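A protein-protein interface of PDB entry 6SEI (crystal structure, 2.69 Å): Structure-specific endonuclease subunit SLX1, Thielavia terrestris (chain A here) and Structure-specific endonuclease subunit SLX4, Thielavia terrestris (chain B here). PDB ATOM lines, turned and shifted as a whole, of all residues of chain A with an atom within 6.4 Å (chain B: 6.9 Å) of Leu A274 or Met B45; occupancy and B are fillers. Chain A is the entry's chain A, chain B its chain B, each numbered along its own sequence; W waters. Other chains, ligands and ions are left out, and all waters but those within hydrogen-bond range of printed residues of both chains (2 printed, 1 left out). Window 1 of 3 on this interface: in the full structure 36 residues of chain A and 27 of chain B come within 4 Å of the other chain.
Of the printed residues of chain B, Leu A274 touches Met B45, Tyr B48 and Ser B87.
Met B45 touches one residue of chain A.
Of the printed residues of chain A, Ser B87 touches Arg A134 (3.1 Å), Trp A135 (2.7 Å) and Leu A274 (3.6 Å).
Of the printed residues of chain B, Ile A273 touches Leu B46, Trp B82 and Val B88.
Printed residues of chain A within 4 Å of Leu B46: Ile A273 (3.3 Å), Pro A275 (3.6 Å) and Trp A289 (2.9 Å).
Of the printed residues of chain B, Trp A289 touches Leu B46 and Tyr B48.
The nearest residue of chain A that does not touch Met B45 is Ile A273 (4.2 Å).
Among the printed residues, merely in contact across the chains: Leu A274 with Met B45, Trp A289 with Tyr B48, Ile A273 with Leu B46, Leu A274 with Ser B87, Pro A275 with Leu B46, Pro A136 with Tyr B48, Leu A274 with Tyr B48, Trp A135 with Cys B89, Ile A273 with Trp B82 and Ile A273 with Val B88.
Water W2 lies within hydrogen-bond range of O of Lys B86 (2.4 Å), N of Ile A273 (3.0 Å) and N of Leu A274 (3.3 Å).
Water W1 bridges O of Ile A273 and NE2 of His B42.
Of the 20 printed residues of chain B, 7 touch a printed residue of chain A.
Hydrophobic or aromatic side chains of chain B that line the printed part of chain A: Leu B46, Tyr B48, Trp B82 and Val B88.
Among the printed residues, 13 pairs touch across the chains.
The backbone NH (N) of Arg A134 is in hydrogen-bond range of the side-chain hydroxyl (OG) of Ser B87 (3.1 Å).
The indole nitrogen of Trp A135 lies within hydrogen-bond range of the backbone carbonyl oxygen of Ser B87 (2.7 Å).
The indole nitrogen (NE1) of Trp A289 sits at hydrogen-bond distance from the backbone carbonyl oxygen (O) of Leu B46 (2.9 Å).
NH1 of Arg A134 lies within hydrogen-bond range of OG of Ser A272, at 3.4 Å.
The backbone carbonyl oxygen of Leu A274 sits at hydrogen-bond distance from the guanidinium group of Arg A134, 2.4 Å away.
The backbone NH (N) of Trp A289 sits at hydrogen-bond distance from the backbone carbonyl oxygen (O) of Val A276, 2.9 Å away.
The backbone NH of Ile B51 is in hydrogen-bond range of the backbone carbonyl oxygen of Cys B89 (2.8 Å).
N of Val B88 lies within hydrogen-bond range of O of Cys B83.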
ATOM      1  N   ARG A 134      -5.327   3.891   6.252  1.00  0.00           N
ATOM      2  CA  ARG A 134      -4.967   5.174   6.844  1.00  0.00           C
ATOM      3  C   ARG A 134      -5.092   5.185   8.365  1.00  0.00           C
ATOM      4  O   ARG A 134      -5.149   6.263   8.968  1.00  0.00           O
ATOM      5  CB  ARG A 134      -5.812   6.286   6.224  1.00  0.00           C
ATOM      6  CG  ARG A 134      -5.793   6.260   4.711  1.00  0.00           C
ATOM      7  CD  ARG A 134      -6.887   7.122   4.126  1.00  0.00           C
ATOM      8  NE  ARG A 134      -6.685   8.525   4.456  1.00  0.00           N
ATOM      9  CZ  ARG A 134      -5.889   9.339   3.772  1.00  0.00           C
ATOM     10  NH1 ARG A 134      -5.225   8.889   2.718  1.00  0.00           N
ATOM     11  NH2 ARG A 134      -5.758  10.605   4.141  1.00  0.00           N
ATOM     12  N   TRP A 135      -5.127   4.013   8.994  1.00  0.00           N
ATOM     13  CA  TRP A 135      -5.135   3.949  10.447  1.00  0.00           C
ATOM     14  C   TRP A 135      -3.742   4.269  10.987  1.00  0.00           C
ATOM     15  O   TRP A 135      -2.739   3.897  10.372  1.00  0.00           O
ATOM     16  CB  TRP A 135      -5.571   2.565  10.927  1.00  0.00           C
ATOM     17  CG  TRP A 135      -7.029   2.274  10.737  1.00  0.00           C
ATOM     18  CD1 TRP A 135      -7.928   3.009  10.020  1.00  0.00           C
ATOM     19  CD2 TRP A 135      -7.758   1.155  11.267  1.00  0.00           C
ATOM     20  NE1 TRP A 135      -9.171   2.421  10.072  1.00  0.00           N
ATOM     21  CE2 TRP A 135      -9.093   1.283  10.834  1.00  0.00           C
ATOM     22  CE3 TRP A 135      -7.411   0.064  12.070  1.00  0.00           C
ATOM     23  CZ2 TRP A 135     -10.079   0.362  11.177  1.00  0.00           C
ATOM     24  CZ3 TRP A 135      -8.389  -0.848  12.407  1.00  0.00           C
ATOM     25  CH2 TRP A 135      -9.708  -0.692  11.966  1.00  0.00           C
ATOM     26  N   PRO A 136      -3.648   4.946  12.139  1.00  0.00           N
ATOM     27  CA  PRO A 136      -2.332   5.340  12.666  1.00  0.00           C
ATOM     28  C   PRO A 136      -1.564   4.177  13.270  1.00  0.00           C
ATOM     29  O   PRO A 136      -1.283   4.167  14.473  1.00  0.00           O
ATOM     30  CB  PRO A 136      -2.690   6.379  13.732  1.00  0.00           C
ATOM     31  CG  PRO A 136      -4.033   5.931  14.223  1.00  0.00           C
ATOM     32  CD  PRO A 136      -4.748   5.365  13.025  1.00  0.00           C
ATOM     33  N   LEU A 265      -5.041  17.387   4.696  1.00  0.00           N
ATOM     34  CA  LEU A 265      -5.489  16.731   3.478  1.00  0.00           C
ATOM     35  C   LEU A 265      -5.437  17.637   2.256  1.00  0.00           C
ATOM     36  O   LEU A 265      -5.794  17.190   1.163  1.00  0.00           O
ATOM     37  CB  LEU A 265      -6.915  16.207   3.676  1.00  0.00           C
ATOM     38  CG  LEU A 265      -7.023  14.965   4.563  1.00  0.00           C
ATOM     39  CD1 LEU A 265      -8.459  14.702   4.971  1.00  0.00           C
ATOM     40  CD2 LEU A 265      -6.446  13.761   3.853  1.00  0.00           C
ATOM     41  N   SER A 272     -10.115  11.969   0.443  1.00  0.00           N
ATOM     42  CA  SER A 272      -9.931  11.332   1.738  1.00  0.00           C
ATOM     43  C   SER A 272     -10.711  12.027   2.855  1.00  0.00           C
ATOM     44  O   SER A 272     -11.128  13.182   2.745  1.00  0.00           O
ATOM     45  CB  SER A 272      -8.447  11.289   2.095  1.00  0.00           C
ATOM     46  OG  SER A 272      -7.697  10.625   1.092  1.00  0.00           O
ATOM     47  N   ILE A 273     -10.906  11.285   3.942  1.00  0.00           N
ATOM     48  CA  ILE A 273     -11.495  11.796   5.174  1.00  0.00           C
ATOM     49  C   ILE A 273     -10.459  11.850   6.294  1.00  0.00           C
ATOM     50  O   ILE A 273     -10.348  12.853   7.002  1.00  0.00           O
ATOM     51  CB  ILE A 273     -12.719  10.946   5.593  1.00  0.00           C
ATOM     52  CG1 ILE A 273     -13.958  11.294   4.752  1.00  0.00           C
ATOM     53  CG2 ILE A 273     -12.981  11.056   7.104  1.00  0.00           C
ATOM     54  CD1 ILE A 273     -14.829  12.398   5.322  1.00  0.00           C
ATOM     55  N   LEU A 274      -9.675  10.782   6.447  1.00  0.00           N
ATOM     56  CA  LEU A 274      -8.768  10.632   7.576  1.00  0.00           C
ATOM     57  C   LEU A 274      -7.385  11.161   7.223  1.00  0.00           C
ATOM     58  O   LEU A 274      -6.711  10.571   6.363  1.00  0.00           O
ATOM     59  CB  LEU A 274      -8.670   9.170   7.984  1.00  0.00           C
ATOM     60  CG  LEU A 274      -9.765   8.618   8.886  1.00  0.00           C
ATOM     61  CD1 LEU A 274      -9.343   7.274   9.460  1.00  0.00           C
ATOM     62  CD2 LEU A 274     -10.069   9.611   9.992  1.00  0.00           C
ATOM     63  N   PRO A 275      -6.908  12.231   7.860  1.00  0.00           N
ATOM     64  CA  PRO A 275      -5.514  12.632   7.667  1.00  0.00           C
ATOM     65  C   PRO A 275      -4.578  11.572   8.224  1.00  0.00           C
ATOM     66  O   PRO A 275      -4.955  10.745   9.059  1.00  0.00           O
ATOM     67  CB  PRO A 275      -5.403  13.947   8.452  1.00  0.00           C
ATOM     68  CG  PRO A 275      -6.813  14.364   8.730  1.00  0.00           C
ATOM     69  CD  PRO A 275      -7.608  13.113   8.805  1.00  0.00           C
ATOM     70  N   VAL A 276      -3.342  11.592   7.738  1.00  0.00           N
ATOM     71  CA  VAL A 276      -2.341  10.633   8.187  1.00  0.00           C
ATOM     72  C   VAL A 276      -1.148  11.409   8.719  1.00  0.00           C
ATOM     73  O   VAL A 276      -0.779  11.277   9.891  1.00  0.00           O
ATOM     74  CB  VAL A 276      -1.923   9.675   7.054  1.00  0.00           C
ATOM     75  CG1 VAL A 276      -0.760   8.811   7.496  1.00  0.00           C
ATOM     76  CG2 VAL A 276      -3.096   8.800   6.621  1.00  0.00           C
ATOM     77  N   TRP A 289      -1.406  12.473  12.447  1.00  0.00           N
ATOM     78  CA  TRP A 289      -2.776  12.755  12.859  1.00  0.00           C
ATOM     79  C   TRP A 289      -3.188  11.914  14.058  1.00  0.00           C
ATOM     80  O   TRP A 289      -3.958  12.377  14.905  1.00  0.00           O
ATOM     81  CB  TRP A 289      -3.727  12.515  11.691  1.00  0.00           C
ATOM     82  CG  TRP A 289      -5.132  12.908  11.974  1.00  0.00           C
ATOM     83  CD1 TRP A 289      -6.169  12.075  12.270  1.00  0.00           C
ATOM     84  CD2 TRP A 289      -5.669  14.236  11.980  1.00  0.00           C
ATOM     85  NE1 TRP A 289      -7.317  12.801  12.467  1.00  0.00           N
ATOM     86  CE2 TRP A 289      -7.037  14.131  12.290  1.00  0.00           C
ATOM     87  CE3 TRP A 289      -5.125  15.502  11.752  1.00  0.00           C
ATOM     88  CZ2 TRP A 289      -7.868  15.245  12.380  1.00  0.00           C
ATOM     89  CZ3 TRP A 289      -5.953  16.604  11.840  1.00  0.00           C
ATOM     90  CH2 TRP A 289      -7.308  16.468  12.155  1.00  0.00           C
ATOM     91  N   ILE B  23     -22.252  11.519  -0.106  1.00  0.00           N
ATOM     92  CA  ILE B  23     -22.114  11.215   1.314  1.00  0.00           C
ATOM     93  C   ILE B  23     -20.955  11.998   1.914  1.00  0.00           C
ATOM     94  O   ILE B  23     -21.070  12.569   3.007  1.00  0.00           O
ATOM     95  CB  ILE B  23     -21.937   9.701   1.532  1.00  0.00           C
ATOM     96  CG1 ILE B  23     -23.107   8.924   0.934  1.00  0.00           C
ATOM     97  CG2 ILE B  23     -21.799   9.390   3.014  1.00  0.00           C
ATOM     98  CD1 ILE B  23     -22.874   7.437   0.903  1.00  0.00           C
ATOM     99  N   VAL B  27     -21.338  14.751   4.986  1.00  0.00           N
ATOM    100  CA  VAL B  27     -20.614  14.676   6.254  1.00  0.00           C
ATOM    101  C   VAL B  27     -19.716  15.896   6.427  1.00  0.00           C
ATOM    102  O   VAL B  27     -19.719  16.551   7.475  1.00  0.00           O
ATOM    103  CB  VAL B  27     -19.800  13.370   6.324  1.00  0.00           C
ATOM    104  CG1 VAL B  27     -18.988  13.309   7.608  1.00  0.00           C
ATOM    105  CG2 VAL B  27     -20.709  12.158   6.201  1.00  0.00           C
ATOM    106  N   SER B  40     -19.656  16.506  15.693  1.00  0.00           N
ATOM    107  CA  SER B  40     -20.370  16.128  14.486  1.00  0.00           C
ATOM    108  C   SER B  40     -19.867  14.778  13.985  1.00  0.00           C
ATOM    109  O   SER B  40     -18.826  14.273  14.414  1.00  0.00           O
ATOM    110  CB  SER B  40     -20.195  17.193  13.406  1.00  0.00           C
ATOM    111  OG  SER B  40     -18.902  17.121  12.829  1.00  0.00           O
ATOM    112  N   TRP B  41     -20.623  14.188  13.056  1.00  0.00           N
ATOM    113  CA  TRP B  41     -20.216  12.905  12.491  1.00  0.00           C
ATOM    114  C   TRP B  41     -18.836  12.999  11.857  1.00  0.00           C
ATOM    115  O   TRP B  41     -18.036  12.061  11.954  1.00  0.00           O
ATOM    116  CB  TRP B  41     -21.246  12.421  11.468  1.00  0.00           C
ATOM    117  CG  TRP B  41     -22.467  11.822  12.093  1.00  0.00           C
ATOM    118  CD1 TRP B  41     -23.744  12.301  12.022  1.00  0.00           C
ATOM    119  CD2 TRP B  41     -22.528  10.633  12.895  1.00  0.00           C
ATOM    120  NE1 TRP B  41     -24.596  11.484  12.726  1.00  0.00           N
ATOM    121  CE2 TRP B  41     -23.874  10.454  13.272  1.00  0.00           C
ATOM    122  CE3 TRP B  41     -21.576   9.705  13.328  1.00  0.00           C
ATOM    123  CZ2 TRP B  41     -24.289   9.388  14.063  1.00  0.00           C
ATOM    124  CZ3 TRP B  41     -21.991   8.647  14.109  1.00  0.00           C
ATOM    125  CH2 TRP B  41     -23.335   8.497  14.469  1.00  0.00           C
ATOM    126  N   HIS B  42     -18.536  14.130  11.213  1.00  0.00           N
ATOM    127  CA  HIS B  42     -17.213  14.326  10.633  1.00  0.00           C
ATOM    128  C   HIS B  42     -16.138  14.339  11.709  1.00  0.00           C
ATOM    129  O   HIS B  42     -15.067  13.745  11.537  1.00  0.00           O
ATOM    130  CB  HIS B  42     -17.189  15.628   9.831  1.00  0.00           C
ATOM    131  CG  HIS B  42     -15.908  15.868   9.092  1.00  0.00           C
ATOM    132  ND1 HIS B  42     -15.502  17.125   8.700  1.00  0.00           N
ATOM    133  CD2 HIS B  42     -14.948  15.013   8.665  1.00  0.00           C
ATOM    134  CE1 HIS B  42     -14.345  17.036   8.069  1.00  0.00           C
ATOM    135  NE2 HIS B  42     -13.988  15.764   8.032  1.00  0.00           N
ATOM    136  N   GLU B  43     -16.408  15.002  12.835  1.00  0.00           N
ATOM    137  CA  GLU B  43     -15.413  15.071  13.898  1.00  0.00           C
ATOM    138  C   GLU B  43     -15.288  13.745  14.636  1.00  0.00           C
ATOM    139  O   GLU B  43     -14.226  13.445  15.193  1.00  0.00           O
ATOM    140  CB  GLU B  43     -15.760  16.207  14.861  1.00  0.00           C
ATOM    141  CG  GLU B  43     -15.629  17.584  14.228  1.00  0.00           C
ATOM    142  CD  GLU B  43     -16.291  18.677  15.044  1.00  0.00           C
ATOM    143  OE1 GLU B  43     -17.431  18.464  15.507  1.00  0.00           O
ATOM    144  OE2 GLU B  43     -15.674  19.753  15.214  1.00  0.00           O
ATOM    145  N   LYS B  44     -16.352  12.940  14.650  1.00  0.00           N
ATOM    146  CA  LYS B  44     -16.236  11.596  15.205  1.00  0.00           C
ATOM    147  C   LYS B  44     -15.276  10.750  14.379  1.00  0.00           C
ATOM    148  O   LYS B  44     -14.446  10.018  14.931  1.00  0.00           O
ATOM    149  CB  LYS B  44     -17.614  10.938  15.286  1.00  0.00           C
ATOM    150  CG  LYS B  44     -18.515  11.531  16.360  1.00  0.00           C
ATOM    151  CD  LYS B  44     -19.830  10.776  16.478  1.00  0.00           C
ATOM    152  CE  LYS B  44     -19.609   9.362  16.987  1.00  0.00           C
ATOM    153  NZ  LYS B  44     -18.954   9.357  18.321  1.00  0.00           N
ATOM    154  N   MET B  45     -15.357  10.856  13.051  1.00  0.00           N
ATOM    155  CA  MET B  45     -14.460  10.092  12.192  1.00  0.00           C
ATOM    156  C   MET B  45     -13.018  10.555  12.350  1.00  0.00           C
ATOM    157  O   MET B  45     -12.105   9.727  12.441  1.00  0.00           O
ATOM    158  CB  MET B  45     -14.910  10.207  10.738  1.00  0.00           C
ATOM    159  CG  MET B  45     -16.319   9.703  10.513  1.00  0.00           C
ATOM    160  SD  MET B  45     -16.994  10.106   8.896  1.00  0.00           S
ATOM    161  CE  MET B  45     -18.717   9.687   9.153  1.00  0.00           C
ATOM    162  N   LEU B  46     -12.794  11.870  12.392  1.00  0.00           N
ATOM    163  CA  LEU B  46     -11.437  12.384  12.552  1.00  0.00           C
ATOM    164  C   LEU B  46     -10.805  11.920  13.857  1.00  0.00           C
ATOM    165  O   LEU B  46      -9.582  11.757  13.928  1.00  0.00           O
ATOM    166  CB  LEU B  46     -11.440  13.911  12.482  1.00  0.00           C
ATOM    167  CG  LEU B  46     -11.815  14.509  11.128  1.00  0.00           C
ATOM    168  CD1 LEU B  46     -11.842  16.027  11.201  1.00  0.00           C
ATOM    169  CD2 LEU B  46     -10.847  14.038  10.058  1.00  0.00           C
ATOM    170  N   MET B  47     -11.610  11.699  14.892  1.00  0.00           N
ATOM    171  CA  MET B  47     -11.114  11.211  16.173  1.00  0.00           C
ATOM    172  C   MET B  47     -11.186   9.695  16.291  1.00  0.00           C
ATOM    173  O   MET B  47     -10.981   9.162  17.386  1.00  0.00           O
ATOM    174  CB  MET B  47     -11.895  11.858  17.320  1.00  0.00           C
ATOM    175  CG  MET B  47     -11.786  13.374  17.369  1.00  0.00           C
ATOM    176  SD  MET B  47     -12.579  14.076  18.829  1.00  0.00           S
ATOM    177  CE  MET B  47     -14.300  13.719  18.473  1.00  0.00           C
ATOM    178  N   TYR B  48     -11.480   8.997  15.190  1.00  0.00           N
ATOM    179  CA  TYR B  48     -11.575   7.534  15.145  1.00  0.00           C
ATOM    180  C   TYR B  48     -12.659   6.984  16.070  1.00  0.00           C
ATOM    181  O   TYR B  48     -12.527   5.876  16.596  1.00  0.00           O
ATOM    182  CB  TYR B  48     -10.241   6.859  15.470  1.00  0.00           C
ATOM    183  CG  TYR B  48      -9.027   7.406  14.758  1.00  0.00           C
ATOM    184  CD1 TYR B  48      -8.808   7.152  13.407  1.00  0.00           C
ATOM    185  CD2 TYR B  48      -8.079   8.152  15.446  1.00  0.00           C
ATOM    186  CE1 TYR B  48      -7.684   7.645  12.762  1.00  0.00           C
ATOM    187  CE2 TYR B  48      -6.957   8.646  14.814  1.00  0.00           C
ATOM    188  CZ  TYR B  48      -6.763   8.393  13.474  1.00  0.00           C
ATOM    189  OH  TYR B  48      -5.640   8.894  12.858  1.00  0.00           O
ATOM    190  N   ASP B  49     -13.732   7.734  16.289  1.00  0.00           N
ATOM    191  CA  ASP B  49     -14.899   7.155  16.939  1.00  0.00           C
ATOM    192  C   ASP B  49     -15.417   6.007  16.079  1.00  0.00           C
ATOM    193  O   ASP B  49     -15.674   6.215  14.883  1.00  0.00           O
ATOM    194  CB  ASP B  49     -16.007   8.192  17.128  1.00  0.00           C
ATOM    195  CG  ASP B  49     -15.714   9.192  18.236  1.00  0.00           C
ATOM    196  OD1 ASP B  49     -14.878   8.905  19.123  1.00  0.00           O
ATOM    197  OD2 ASP B  49     -16.339  10.274  18.220  1.00  0.00           O
ATOM    198  N   ILE B  51     -17.909   4.115  14.174  1.00  0.00           N
ATOM    199  CA  ILE B  51     -19.122   4.707  13.619  1.00  0.00           C
ATOM    200  C   ILE B  51     -20.234   3.664  13.625  1.00  0.00           C
ATOM    201  O   ILE B  51     -20.168   2.663  12.908  1.00  0.00           O
ATOM    202  CB  ILE B  51     -18.878   5.245  12.204  1.00  0.00           C
ATOM    203  CG1 ILE B  51     -17.811   6.340  12.237  1.00  0.00           C
ATOM    204  CG2 ILE B  51     -20.168   5.766  11.596  1.00  0.00           C
ATOM    205  CD1 ILE B  51     -18.108   7.451  13.215  1.00  0.00           C
ATOM    206  N   LEU B  56     -25.346   6.879  11.603  1.00  0.00           N
ATOM    207  CA  LEU B  56     -24.968   7.743  10.490  1.00  0.00           C
ATOM    208  C   LEU B  56     -25.908   7.549   9.307  1.00  0.00           C
ATOM    209  O   LEU B  56     -26.246   8.513   8.608  1.00  0.00           O
ATOM    210  CB  LEU B  56     -23.521   7.476  10.074  1.00  0.00           C
ATOM    211  CG  LEU B  56     -23.043   8.285   8.863  1.00  0.00           C
ATOM    212  CD1 LEU B  56     -22.956   9.766   9.204  1.00  0.00           C
ATOM    213  CD2 LEU B  56     -21.713   7.769   8.337  1.00  0.00           C
ATOM    214  N   TRP B  82     -18.947   2.881   2.081  1.00  0.00           N
ATOM    215  CA  TRP B  82     -18.303   4.191   2.064  1.00  0.00           C
ATOM    216  C   TRP B  82     -17.267   4.308   3.174  1.00  0.00           C
ATOM    217  O   TRP B  82     -16.142   4.762   2.941  1.00  0.00           O
ATOM    218  CB  TRP B  82     -19.353   5.295   2.196  1.00  0.00           C
ATOM    219  CG  TRP B  82     -18.775   6.685   2.162  1.00  0.00           C
ATOM    220  CD1 TRP B  82     -18.523   7.444   1.052  1.00  0.00           C
ATOM    221  CD2 TRP B  82     -18.374   7.481   3.288  1.00  0.00           C
ATOM    222  NE1 TRP B  82     -17.991   8.658   1.418  1.00  0.00           N
ATOM    223  CE2 TRP B  82     -17.888   8.705   2.784  1.00  0.00           C
ATOM    224  CE3 TRP B  82     -18.377   7.275   4.673  1.00  0.00           C
ATOM    225  CZ2 TRP B  82     -17.415   9.717   3.613  1.00  0.00           C
ATOM    226  CZ3 TRP B  82     -17.905   8.281   5.494  1.00  0.00           C
ATOM    227  CH2 TRP B  82     -17.432   9.487   4.962  1.00  0.00           C
ATOM    228  N   CYS B  83     -17.631   3.897   4.391  1.00  0.00           N
ATOM    229  CA  CYS B  83     -16.704   3.992   5.515  1.00  0.00           C
ATOM    230  C   CYS B  83     -15.450   3.171   5.259  1.00  0.00           C
ATOM    231  O   CYS B  83     -14.326   3.643   5.473  1.00  0.00           O
ATOM    232  CB  CYS B  83     -17.384   3.523   6.800  1.00  0.00           C
ATOM    233  SG  CYS B  83     -18.646   4.635   7.437  1.00  0.00           S
ATOM    234  N   LYS B  86     -13.087   4.684   3.090  1.00  0.00           N
ATOM    235  CA  LYS B  86     -12.473   5.872   3.674  1.00  0.00           C
ATOM    236  C   LYS B  86     -11.574   5.571   4.866  1.00  0.00           C
ATOM    237  O   LYS B  86     -11.098   6.512   5.510  1.00  0.00           O
ATOM    238  CB  LYS B  86     -13.552   6.869   4.118  1.00  0.00           C
ATOM    239  CG  LYS B  86     -14.431   7.404   3.010  1.00  0.00           C
ATOM    240  CD  LYS B  86     -13.629   8.160   1.979  1.00  0.00           C
ATOM    241  CE  LYS B  86     -14.546   8.841   0.987  1.00  0.00           C
ATOM    242  NZ  LYS B  86     -13.916   8.926  -0.356  1.00  0.00           N
ATOM    243  N   SER B  87     -11.341   4.295   5.180  1.00  0.00           N
ATOM    244  CA  SER B  87     -10.661   3.844   6.395  1.00  0.00           C
ATOM    245  C   SER B  87     -11.403   4.241   7.664  1.00  0.00           C
ATOM    246  O   SER B  87     -10.854   4.112   8.765  1.00  0.00           O
ATOM    247  CB  SER B  87      -9.211   4.344   6.465  1.00  0.00           C
ATOM    248  OG  SER B  87      -8.318   3.373   5.952  1.00  0.00           O
ATOM    249  N   VAL B  88     -12.638   4.716   7.539  1.00  0.00           N
ATOM    250  CA  VAL B  88     -13.447   5.075   8.697  1.00  0.00           C
ATOM    251  C   VAL B  88     -13.970   3.793   9.332  1.00  0.00           C
ATOM    252  O   VAL B  88     -14.677   3.007   8.691  1.00  0.00           O
ATOM    253  CB  VAL B  88     -14.590   6.019   8.304  1.00  0.00           C
ATOM    254  CG1 VAL B  88     -15.462   6.325   9.505  1.00  0.00           C
ATOM    255  CG2 VAL B  88     -14.028   7.305   7.716  1.00  0.00           C
ATOM    256  N   CYS B  89     -13.604   3.575  10.592  1.00  0.00           N
ATOM    257  CA  CYS B  89     -13.984   2.376  11.323  1.00  0.00           C
ATOM    258  C   CYS B  89     -15.451   2.440  11.730  1.00  0.00           C
ATOM    259  O   CYS B  89     -15.890   3.418  12.345  1.00  0.00           O
ATOM    260  CB  CYS B  89     -13.089   2.242  12.555  1.00  0.00           C
ATOM    261  SG  CYS B  89     -13.559   1.008  13.777  1.00  0.00           S
HETATM  262  O   HOH W   1     -11.312  15.573   6.325  1.00  0.00           O
HETATM  263  O   HOH W   2     -10.196   8.384   4.249  1.00  0.00           O
